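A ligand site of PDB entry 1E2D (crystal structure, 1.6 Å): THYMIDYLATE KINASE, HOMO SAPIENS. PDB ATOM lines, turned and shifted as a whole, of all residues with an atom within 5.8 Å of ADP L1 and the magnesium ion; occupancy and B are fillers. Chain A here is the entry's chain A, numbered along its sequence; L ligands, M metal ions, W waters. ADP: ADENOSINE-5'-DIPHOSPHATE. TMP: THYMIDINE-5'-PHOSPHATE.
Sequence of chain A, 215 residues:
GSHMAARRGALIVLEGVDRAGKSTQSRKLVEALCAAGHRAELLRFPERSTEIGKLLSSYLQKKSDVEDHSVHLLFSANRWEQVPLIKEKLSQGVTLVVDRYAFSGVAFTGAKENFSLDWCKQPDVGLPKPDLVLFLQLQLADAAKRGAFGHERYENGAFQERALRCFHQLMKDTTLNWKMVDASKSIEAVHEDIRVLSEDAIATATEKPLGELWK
N of Ser 23 sits at hydrogen-bond distance from O2A of ADP L1 (3.5 Å). An oxygen (O2A) of ADP L1 is in hydrogen-bond range of the backbone NH (N) of Thr 24 (2.8 Å). The side-chain hydroxyl of Thr 24 is in hydrogen-bond range of an oxygen (O2A) of ADP L1, at 2.7 Å. The backbone NH of Lys 22 lies within hydrogen-bond range of an oxygen (O1B) of ADP L1 (2.8 Å). An oxygen (O1B) of ADP L1 is in salt-bridge range of the side-chain amino group (NZ) of Lys 22, at 2.7 Å. The backbone carbonyl oxygen (O) of Lys 185 is in hydrogen-bond range of a nitrogen (N6) of ADP L1 (2.8 Å). N of Gly 21 lies within hydrogen-bond range of O1B of ADP L1 (3.0 Å). The guanidinium group of Arg 146 lies close to a nitrogen (N1) of ADP L1. O3B of ADP L1 is in hydrogen-bond range of N of Arg 19 (3.3 Å). The backbone NH (N) of Ala 20 sits at hydrogen-bond distance from an oxygen (O1B) of ADP L1. An oxygen (O2P) of TMP L2 is in salt-bridge range of the guanidinium group (NE) of Arg 100.
OD2 of Asp 99 lies close to OG of Ser 23 (2.6 Å). NH2 of Arg 27 sits at hydrogen-bond distance from OG1 of Thr 24 (3.2 Å). NZ of Lys 22 sits at hydrogen-bond distance from O of Val 17 (3.2 Å). The guanidinium group of Arg 146 sits at hydrogen-bond distance from the backbone carbonyl oxygen of Arg 19 (3.1 Å). The guanidinium group (NH1) of Arg 146 is in hydrogen-bond range of the backbone carbonyl oxygen (O) of Ala 20 (3.0 Å). The guanidinium group (NH2) of Arg 146 is in hydrogen-bond range of the backbone carbonyl oxygen (O) of Ala 183 (2.7 Å). OD2 of Asp 18 lies within salt-bridge range of NE of Arg 19, at 3.4 Å. The backbone carbonyl oxygen of Ile 187 lies within hydrogen-bond range of the side-chain amide nitrogen of Gln 25 (3.2 Å).
Merely in contact with ADP L1: Ile 187, Ser 186, Ala 183 and Val 17. Hydrophobic or aromatic side chains that line ADP L1: Ile 187. Of the 20 residues printed, 12 come within 4 Å of ADP L1. The nearest printed residue that does not touch ADP L1 is Val 190 (4.05 Å).
One residue has an atom within 4 Å of the magnesium ion: Ser 23.
The magnesium ion is bound by an oxygen (O2B) of ADP L1 (2.0 Å), water W14 (2.1 Å), water W13 (2.1 Å), water W5 (2.1 Å), water W11 (2.1 Å) and the side-chain hydroxyl of Ser 23 (2.1 Å).
Water W5 bridges O2P of TMP L2 and OD1 of Asp 99. Water W15 lies within hydrogen-bond range of O2' of ADP L1 and OG1 of Thr 24. Water W3 lies within hydrogen-bond range of N7 of ADP L1 (2.8 Å), NE2 of Gln 25 (2.9 Å) and O of Ala 20 (3.1 Å). Water W10 lies within hydrogen-bond range of NH2 of Arg 27, O1A of ADP L1 and OG1 of Thr 24. Water W7 lies within hydrogen-bond range of the side-chain carboxylate (OD1) of Asp 18 (2.5 Å), the side-chain amino group (NZ) of Lys 22 (2.9 Å), an oxygen (O3B) of ADP L1 (3.0 Å) and the guanidinium group (NH2) of Arg 100 (3.1 Å). Water W1 lies within hydrogen-bond range of O of Arg 146 (2.8 Å) and O3' of ADP L1 (3.5 Å).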
ATOM      1  N   GLY A  16     -36.857 -28.288   9.831  1.00  0.00           N
ATOM      2  CA  GLY A  16     -36.121 -28.886   8.713  1.00  0.00           C
ATOM      3  C   GLY A  16     -35.794 -30.356   9.020  1.00  0.00           C
ATOM      4  O   GLY A  16     -35.981 -30.824  10.153  1.00  0.00           O
ATOM      5  N   VAL A  17     -35.299 -31.044   7.998  1.00  0.00           N
ATOM      6  CA  VAL A  17     -34.958 -32.457   8.164  1.00  0.00           C
ATOM      7  C   VAL A  17     -33.680 -32.611   8.959  1.00  0.00           C
ATOM      8  O   VAL A  17     -32.930 -31.643   9.172  1.00  0.00           O
ATOM      9  CB  VAL A  17     -34.865 -33.150   6.790  1.00  0.00           C
ATOM     10  CG1 VAL A  17     -36.253 -33.036   6.158  1.00  0.00           C
ATOM     11  CG2 VAL A  17     -33.804 -32.479   5.967  1.00  0.00           C
ATOM     12  N   ASP A  18     -33.471 -33.829   9.438  1.00  0.00           N
ATOM     13  CA  ASP A  18     -32.304 -34.099  10.279  1.00  0.00           C
ATOM     14  C   ASP A  18     -31.016 -33.690   9.583  1.00  0.00           C
ATOM     15  O   ASP A  18     -30.787 -34.042   8.427  1.00  0.00           O
ATOM     16  CB  ASP A  18     -32.319 -35.580  10.639  1.00  0.00           C
ATOM     17  CG  ASP A  18     -31.372 -35.900  11.791  1.00  0.00           C
ATOM     18  OD1 ASP A  18     -31.238 -35.095  12.732  1.00  0.00           O
ATOM     19  OD2 ASP A  18     -30.755 -36.981  11.698  1.00  0.00           O
ATOM     20  N   ARG A  19     -30.172 -33.001  10.336  1.00  0.00           N
ATOM     21  CA  ARG A  19     -28.867 -32.588   9.905  1.00  0.00           C
ATOM     22  C   ARG A  19     -28.913 -31.523   8.836  1.00  0.00           C
ATOM     23  O   ARG A  19     -27.848 -31.193   8.335  1.00  0.00           O
ATOM     24  CB  ARG A  19     -28.032 -33.764   9.352  1.00  0.00           C
ATOM     25  CG  ARG A  19     -27.793 -34.791  10.450  1.00  0.00           C
ATOM     26  CD  ARG A  19     -26.931 -35.949   9.933  1.00  0.00           C
ATOM     27  NE  ARG A  19     -27.602 -37.187  10.351  1.00  0.00           N
ATOM     28  CZ  ARG A  19     -27.701 -38.302   9.631  1.00  0.00           C
ATOM     29  NH1 ARG A  19     -27.160 -38.418   8.432  1.00  0.00           N
ATOM     30  NH2 ARG A  19     -28.384 -39.311  10.165  1.00  0.00           N
ATOM     31  N   ALA A  20     -30.105 -31.000   8.559  1.00  0.00           N
ATOM     32  CA  ALA A  20     -30.172 -29.968   7.507  1.00  0.00           C
ATOM     33  C   ALA A  20     -29.459 -28.695   7.919  1.00  0.00           C
ATOM     34  O   ALA A  20     -29.032 -27.932   7.062  1.00  0.00           O
ATOM     35  CB  ALA A  20     -31.639 -29.701   7.208  1.00  0.00           C
ATOM     36  N   GLY A  21     -29.340 -28.475   9.233  1.00  0.00           N
ATOM     37  CA  GLY A  21     -28.632 -27.346   9.750  1.00  0.00           C
ATOM     38  C   GLY A  21     -29.460 -26.356  10.555  1.00  0.00           C
ATOM     39  O   GLY A  21     -29.101 -25.187  10.639  1.00  0.00           O
ATOM     40  N   LYS A  22     -30.529 -26.819  11.184  1.00  0.00           N
ATOM     41  CA  LYS A  22     -31.346 -25.911  11.983  1.00  0.00           C
ATOM     42  C   LYS A  22     -30.538 -25.185  13.054  1.00  0.00           C
ATOM     43  O   LYS A  22     -30.673 -23.980  13.331  1.00  0.00           O
ATOM     44  CB  LYS A  22     -32.433 -26.749  12.711  1.00  0.00           C
ATOM     45  CG  LYS A  22     -33.469 -27.305  11.729  1.00  0.00           C
ATOM     46  CD  LYS A  22     -34.445 -28.210  12.481  1.00  0.00           C
ATOM     47  CE  LYS A  22     -33.805 -29.436  13.123  1.00  0.00           C
ATOM     48  NZ  LYS A  22     -33.272 -30.403  12.085  1.00  0.00           N
ATOM     49  N   SER A  23     -29.733 -25.958  13.777  1.00  0.00           N
ATOM     50  CA  SER A  23     -28.983 -25.314  14.884  1.00  0.00           C
ATOM     51  C   SER A  23     -27.845 -24.410  14.386  1.00  0.00           C
ATOM     52  O   SER A  23     -27.674 -23.301  14.912  1.00  0.00           O
ATOM     53  CB  SER A  23     -28.465 -26.363  15.835  1.00  0.00           C
ATOM     54  OG  SER A  23     -29.566 -27.126  16.350  1.00  0.00           O
ATOM     55  N   THR A  24     -27.184 -24.933  13.361  1.00  0.00           N
ATOM     56  CA  THR A  24     -26.065 -24.152  12.777  1.00  0.00           C
ATOM     57  C   THR A  24     -26.599 -22.821  12.240  1.00  0.00           C
ATOM     58  O   THR A  24     -26.091 -21.734  12.566  1.00  0.00           O
ATOM     59  CB  THR A  24     -25.355 -24.929  11.687  1.00  0.00           C
ATOM     60  OG1 THR A  24     -24.705 -26.060  12.261  1.00  0.00           O
ATOM     61  CG2 THR A  24     -24.318 -24.085  10.962  1.00  0.00           C
ATOM     62  N   GLN A  25     -27.663 -22.933  11.439  1.00  0.00           N
ATOM     63  CA  GLN A  25     -28.216 -21.737  10.845  1.00  0.00           C
ATOM     64  C   GLN A  25     -28.932 -20.822  11.842  1.00  0.00           C
ATOM     65  O   GLN A  25     -28.899 -19.584  11.671  1.00  0.00           O
ATOM     66  CB  GLN A  25     -29.152 -22.063   9.649  1.00  0.00           C
ATOM     67  CG  GLN A  25     -28.435 -22.918   8.610  1.00  0.00           C
ATOM     68  CD  GLN A  25     -27.362 -22.126   7.900  1.00  0.00           C
ATOM     69  OE1 GLN A  25     -27.291 -20.892   7.970  1.00  0.00           O
ATOM     70  NE2 GLN A  25     -26.482 -22.807   7.198  1.00  0.00           N
ATOM     71  N   ARG A  27     -27.978 -20.299  14.936  1.00  0.00           N
ATOM     72  CA  ARG A  27     -26.873 -19.599  15.588  1.00  0.00           C
ATOM     73  C   ARG A  27     -26.288 -18.510  14.692  1.00  0.00           C
ATOM     74  O   ARG A  27     -26.117 -17.398  15.167  1.00  0.00           O
ATOM     75  CB  ARG A  27     -25.667 -20.561  15.877  1.00  0.00           C
ATOM     76  CG  ARG A  27     -25.969 -21.510  17.028  1.00  0.00           C
ATOM     77  CD  ARG A  27     -24.763 -22.327  17.478  1.00  0.00           C
ATOM     78  NE  ARG A  27     -24.186 -23.110  16.372  1.00  0.00           N
ATOM     79  CZ  ARG A  27     -24.419 -24.391  16.112  1.00  0.00           C
ATOM     80  NH1 ARG A  27     -25.297 -25.091  16.817  1.00  0.00           N
ATOM     81  NH2 ARG A  27     -23.757 -24.867  15.074  1.00  0.00           N
ATOM     82  N   ASP A  99     -34.987 -22.489  17.160  1.00  0.00           N
ATOM     83  CA  ASP A  99     -34.571 -23.776  16.620  1.00  0.00           C
ATOM     84  C   ASP A  99     -35.546 -24.859  17.036  1.00  0.00           C
ATOM     85  O   ASP A  99     -35.549 -25.304  18.175  1.00  0.00           O
ATOM     86  CB  ASP A  99     -33.149 -24.001  17.163  1.00  0.00           C
ATOM     87  CG  ASP A  99     -32.488 -25.278  16.737  1.00  0.00           C
ATOM     88  OD1 ASP A  99     -33.048 -26.071  15.953  1.00  0.00           O
ATOM     89  OD2 ASP A  99     -31.348 -25.501  17.238  1.00  0.00           O
ATOM     90  N   ARG A 100     -36.497 -25.145  16.157  1.00  0.00           N
ATOM     91  CA  ARG A 100     -37.654 -25.979  16.332  1.00  0.00           C
ATOM     92  C   ARG A 100     -38.744 -25.289  17.168  1.00  0.00           C
ATOM     93  O   ARG A 100     -38.510 -24.471  18.045  1.00  0.00           O
ATOM     94  CB  ARG A 100     -37.356 -27.311  17.041  1.00  0.00           C
ATOM     95  CG  ARG A 100     -36.466 -28.238  16.221  1.00  0.00           C
ATOM     96  CD  ARG A 100     -36.489 -29.620  16.878  1.00  0.00           C
ATOM     97  NE  ARG A 100     -35.477 -30.558  16.354  1.00  0.00           N
ATOM     98  CZ  ARG A 100     -35.702 -31.341  15.306  1.00  0.00           C
ATOM     99  NH1 ARG A 100     -36.835 -31.343  14.600  1.00  0.00           N
ATOM    100  NH2 ARG A 100     -34.717 -32.179  14.966  1.00  0.00           N
ATOM    101  N   ARG A 146     -23.345 -35.829   6.534  1.00  0.00           N
ATOM    102  CA  ARG A 146     -23.226 -34.896   7.640  1.00  0.00           C
ATOM    103  C   ARG A 146     -23.216 -35.556   9.018  1.00  0.00           C
ATOM    104  O   ARG A 146     -23.003 -34.916  10.054  1.00  0.00           O
ATOM    105  CB  ARG A 146     -24.352 -33.848   7.553  1.00  0.00           C
ATOM    106  CG  ARG A 146     -24.157 -32.884   6.385  1.00  0.00           C
ATOM    107  CD  ARG A 146     -25.291 -31.881   6.287  1.00  0.00           C
ATOM    108  NE  ARG A 146     -25.303 -31.134   5.063  1.00  0.00           N
ATOM    109  CZ  ARG A 146     -26.105 -30.079   4.816  1.00  0.00           C
ATOM    110  NH1 ARG A 146     -26.938 -29.654   5.757  1.00  0.00           N
ATOM    111  NH2 ARG A 146     -26.032 -29.474   3.652  1.00  0.00           N
ATOM    112  N   ALA A 183     -31.159 -26.476   1.888  1.00  0.00           N
ATOM    113  CA  ALA A 183     -30.071 -26.637   2.865  1.00  0.00           C
ATOM    114  C   ALA A 183     -28.926 -27.505   2.357  1.00  0.00           C
ATOM    115  O   ALA A 183     -27.968 -27.750   3.093  1.00  0.00           O
ATOM    116  CB  ALA A 183     -30.682 -27.163   4.162  1.00  0.00           C
ATOM    117  N   SER A 184     -28.980 -27.827   1.050  1.00  0.00           N
ATOM    118  CA  SER A 184     -27.874 -28.636   0.521  1.00  0.00           C
ATOM    119  C   SER A 184     -26.677 -27.769   0.151  1.00  0.00           C
ATOM    120  O   SER A 184     -25.586 -28.320  -0.117  1.00  0.00           O
ATOM    121  CB  SER A 184     -28.352 -29.439  -0.687  1.00  0.00           C
ATOM    122  OG  SER A 184     -28.510 -28.579  -1.798  1.00  0.00           O
ATOM    123  N   LYS A 185     -26.794 -26.453   0.093  1.00  0.00           N
ATOM    124  CA  LYS A 185     -25.640 -25.622  -0.257  1.00  0.00           C
ATOM    125  C   LYS A 185     -24.663 -25.510   0.908  1.00  0.00           C
ATOM    126  O   LYS A 185     -24.908 -26.123   1.932  1.00  0.00           O
ATOM    127  CB  LYS A 185     -26.072 -24.232  -0.727  1.00  0.00           C
ATOM    128  CG  LYS A 185     -27.117 -24.273  -1.871  1.00  0.00           C
ATOM    129  CD  LYS A 185     -27.558 -22.813  -2.015  1.00  0.00           C
ATOM    130  CE  LYS A 185     -28.738 -22.505  -2.887  1.00  0.00           C
ATOM    131  NZ  LYS A 185     -29.147 -21.084  -2.633  1.00  0.00           N
ATOM    132  N   SER A 186     -23.605 -24.733   0.746  1.00  0.00           N
ATOM    133  CA  SER A 186     -22.610 -24.530   1.772  1.00  0.00           C
ATOM    134  C   SER A 186     -23.254 -23.890   2.998  1.00  0.00           C
ATOM    135  O   SER A 186     -24.350 -23.305   2.910  1.00  0.00           O
ATOM    136  CB  SER A 186     -21.436 -23.651   1.325  1.00  0.00           C
ATOM    137  OG  SER A 186     -21.819 -22.295   1.120  1.00  0.00           O
ATOM    138  N   ILE A 187     -22.578 -24.006   4.143  1.00  0.00           N
ATOM    139  CA  ILE A 187     -23.135 -23.364   5.338  1.00  0.00           C
ATOM    140  C   ILE A 187     -23.320 -21.873   5.071  1.00  0.00           C
ATOM    141  O   ILE A 187     -24.317 -21.293   5.463  1.00  0.00           O
ATOM    142  CB  ILE A 187     -22.213 -23.636   6.537  1.00  0.00           C
ATOM    143  CG1 ILE A 187     -22.418 -25.075   7.014  1.00  0.00           C
ATOM    144  CG2 ILE A 187     -22.498 -22.640   7.639  1.00  0.00           C
ATOM    145  CD1 ILE A 187     -21.420 -25.480   8.097  1.00  0.00           C
ATOM    146  N   VAL A 190     -26.300 -21.190   2.499  1.00  0.00           N
ATOM    147  CA  VAL A 190     -27.622 -21.366   3.147  1.00  0.00           C
ATOM    148  C   VAL A 190     -27.903 -20.213   4.114  1.00  0.00           C
ATOM    149  O   VAL A 190     -29.014 -19.728   4.225  1.00  0.00           O
ATOM    150  CB  VAL A 190     -27.642 -22.706   3.892  1.00  0.00           C
ATOM    151  CG1 VAL A 190     -28.978 -22.885   4.659  1.00  0.00           C
ATOM    152  CG2 VAL A 190     -27.439 -23.873   2.942  1.00  0.00           C
HETATM  153  PB  ADP L   1     -29.700 -29.833  12.757  1.00  0.00           P
HETATM  154  O1B ADP L   1     -30.684 -29.581  11.675  1.00  0.00           O
HETATM  155  O2B ADP L   1     -29.838 -29.028  13.970  1.00  0.00           O
HETATM  156  O3B ADP L   1     -29.705 -31.365  13.191  1.00  0.00           O
HETATM  157  PA  ADP L   1     -26.843 -29.085  12.610  1.00  0.00           P
HETATM  158  O1A ADP L   1     -26.483 -29.567  13.968  1.00  0.00           O
HETATM  159  O2A ADP L   1     -26.940 -27.593  12.457  1.00  0.00           O
HETATM  160  O3A ADP L   1     -28.229 -29.716  12.106  1.00  0.00           O
HETATM  161  O5' ADP L   1     -25.820 -29.617  11.551  1.00  0.00           O
HETATM  162  C5' ADP L   1     -25.598 -31.060  11.400  1.00  0.00           C
HETATM  163  C4' ADP L   1     -24.138 -31.241  10.937  1.00  0.00           C
HETATM  164  O4' ADP L   1     -24.034 -30.915   9.544  1.00  0.00           O
HETATM  165  C3' ADP L   1     -23.181 -30.394  11.732  1.00  0.00           C
HETATM  166  O3' ADP L   1     -21.943 -31.074  11.879  1.00  0.00           O
HETATM  167  C2' ADP L   1     -22.958 -29.204  10.762  1.00  0.00           C
HETATM  168  O2' ADP L   1     -21.675 -28.689  10.886  1.00  0.00           O
HETATM  169  C1' ADP L   1     -23.130 -29.857   9.387  1.00  0.00           C
HETATM  170  N9  ADP L   1     -23.739 -28.885   8.458  1.00  0.00           N
HETATM  171  C8  ADP L   1     -24.837 -28.088   8.736  1.00  0.00           C
HETATM  172  N7  ADP L   1     -25.233 -27.394   7.684  1.00  0.00           N
HETATM  173  C5  ADP L   1     -24.338 -27.782   6.641  1.00  0.00           C
HETATM  174  C6  ADP L   1     -24.207 -27.421   5.299  1.00  0.00           C
HETATM  175  N6  ADP L   1     -24.940 -26.545   4.674  1.00  0.00           N
HETATM  176  N1  ADP L   1     -23.190 -28.023   4.672  1.00  0.00           N
HETATM  177  C2  ADP L   1     -22.349 -28.915   5.220  1.00  0.00           C
HETATM  178  N3  ADP L   1     -22.398 -29.307   6.479  1.00  0.00           N
HETATM  179  C4  ADP L   1     -23.397 -28.672   7.103  1.00  0.00           C
HETATM  180  P   TMP L   2     -32.889 -31.395  18.234  1.00  0.00           P
HETATM  181  O1P TMP L   2     -32.677 -32.309  17.058  1.00  0.00           O
HETATM  182  O2P TMP L   2     -33.353 -30.015  17.974  1.00  0.00           O
HETATM  183  O3P TMP L   2     -31.658 -31.526  19.178  1.00  0.00           O
HETATM  184  O5' TMP L   2     -34.126 -31.935  19.113  1.00  0.00           O
HETATM  185  C5' TMP L   2     -34.155 -33.162  19.836  1.00  0.00           C
HETATM  186  C4' TMP L   2     -35.433 -33.943  19.513  1.00  0.00           C
HETATM  187  O4' TMP L   2     -36.733 -33.505  20.037  1.00  0.00           O
HETATM  188  C3' TMP L   2     -35.601 -34.284  18.042  1.00  0.00           C
HETATM  189  O3' TMP L   2     -35.681 -35.704  17.844  1.00  0.00           O
HETATM  190  C2' TMP L   2     -37.002 -33.721  17.725  1.00  0.00           C
HETATM  191  C1' TMP L   2     -37.693 -33.792  19.105  1.00  0.00           C
HETATM  192  N1  TMP L   2     -38.907 -33.031  19.312  1.00  0.00           N
HETATM  193  C2  TMP L   2     -40.109 -33.698  19.639  1.00  0.00           C
HETATM  194  O2  TMP L   2     -40.233 -34.930  19.543  1.00  0.00           O
HETATM  195  N3  TMP L   2     -41.121 -32.827  19.974  1.00  0.00           N
HETATM  196  C4  TMP L   2     -40.992 -31.462  20.088  1.00  0.00           C
HETATM  197  O4  TMP L   2     -42.001 -30.618  20.466  1.00  0.00           O
HETATM  198  C5  TMP L   2     -39.699 -30.847  19.737  1.00  0.00           C
HETATM  199  C5M TMP L   2     -39.538 -29.383  19.888  1.00  0.00           C
HETATM  200  C6  TMP L   2     -38.672 -31.708  19.421  1.00  0.00           C
HETATM  201 MG    MG M   1     -30.037 -29.171  15.990  1.00  0.00          MG
HETATM  202  O   HOH W   1     -20.815 -33.260   9.428  1.00  0.00           O
HETATM  203  O   HOH W   2     -23.117 -28.808   2.111  1.00  0.00           O
HETATM  204  O   HOH W   3     -27.066 -25.561   6.729  1.00  0.00           O
HETATM  205  O   HOH W   4     -27.709 -32.973  13.874  1.00  0.00           O
HETATM  206  O   HOH W   5     -32.076 -28.605  16.108  1.00  0.00           O
HETATM  207  O   HOH W   6     -24.725 -31.318  15.154  1.00  0.00           O
HETATM  208  O   HOH W   7     -32.252 -32.858  13.238  1.00  0.00           O
HETATM  209  O   HOH W   8     -19.398 -27.499   6.053  1.00  0.00           O
HETATM  210  O   HOH W   9     -20.828 -31.607   7.310  1.00  0.00           O
HETATM  211  O   HOH W  10     -24.765 -27.579  15.278  1.00  0.00           O
HETATM  212  O   HOH W  11     -30.601 -31.213  15.825  1.00  0.00           O
HETATM  213  O   HOH W  12     -22.515 -32.601  14.128  1.00  0.00           O
HETATM  214  O   HOH W  13     -30.049 -29.353  18.094  1.00  0.00           O
HETATM  215  O   HOH W  14     -28.048 -29.685  16.165  1.00  0.00           O
HETATM  216  O   HOH W  15     -22.165 -26.938  12.657  1.00  0.00           O
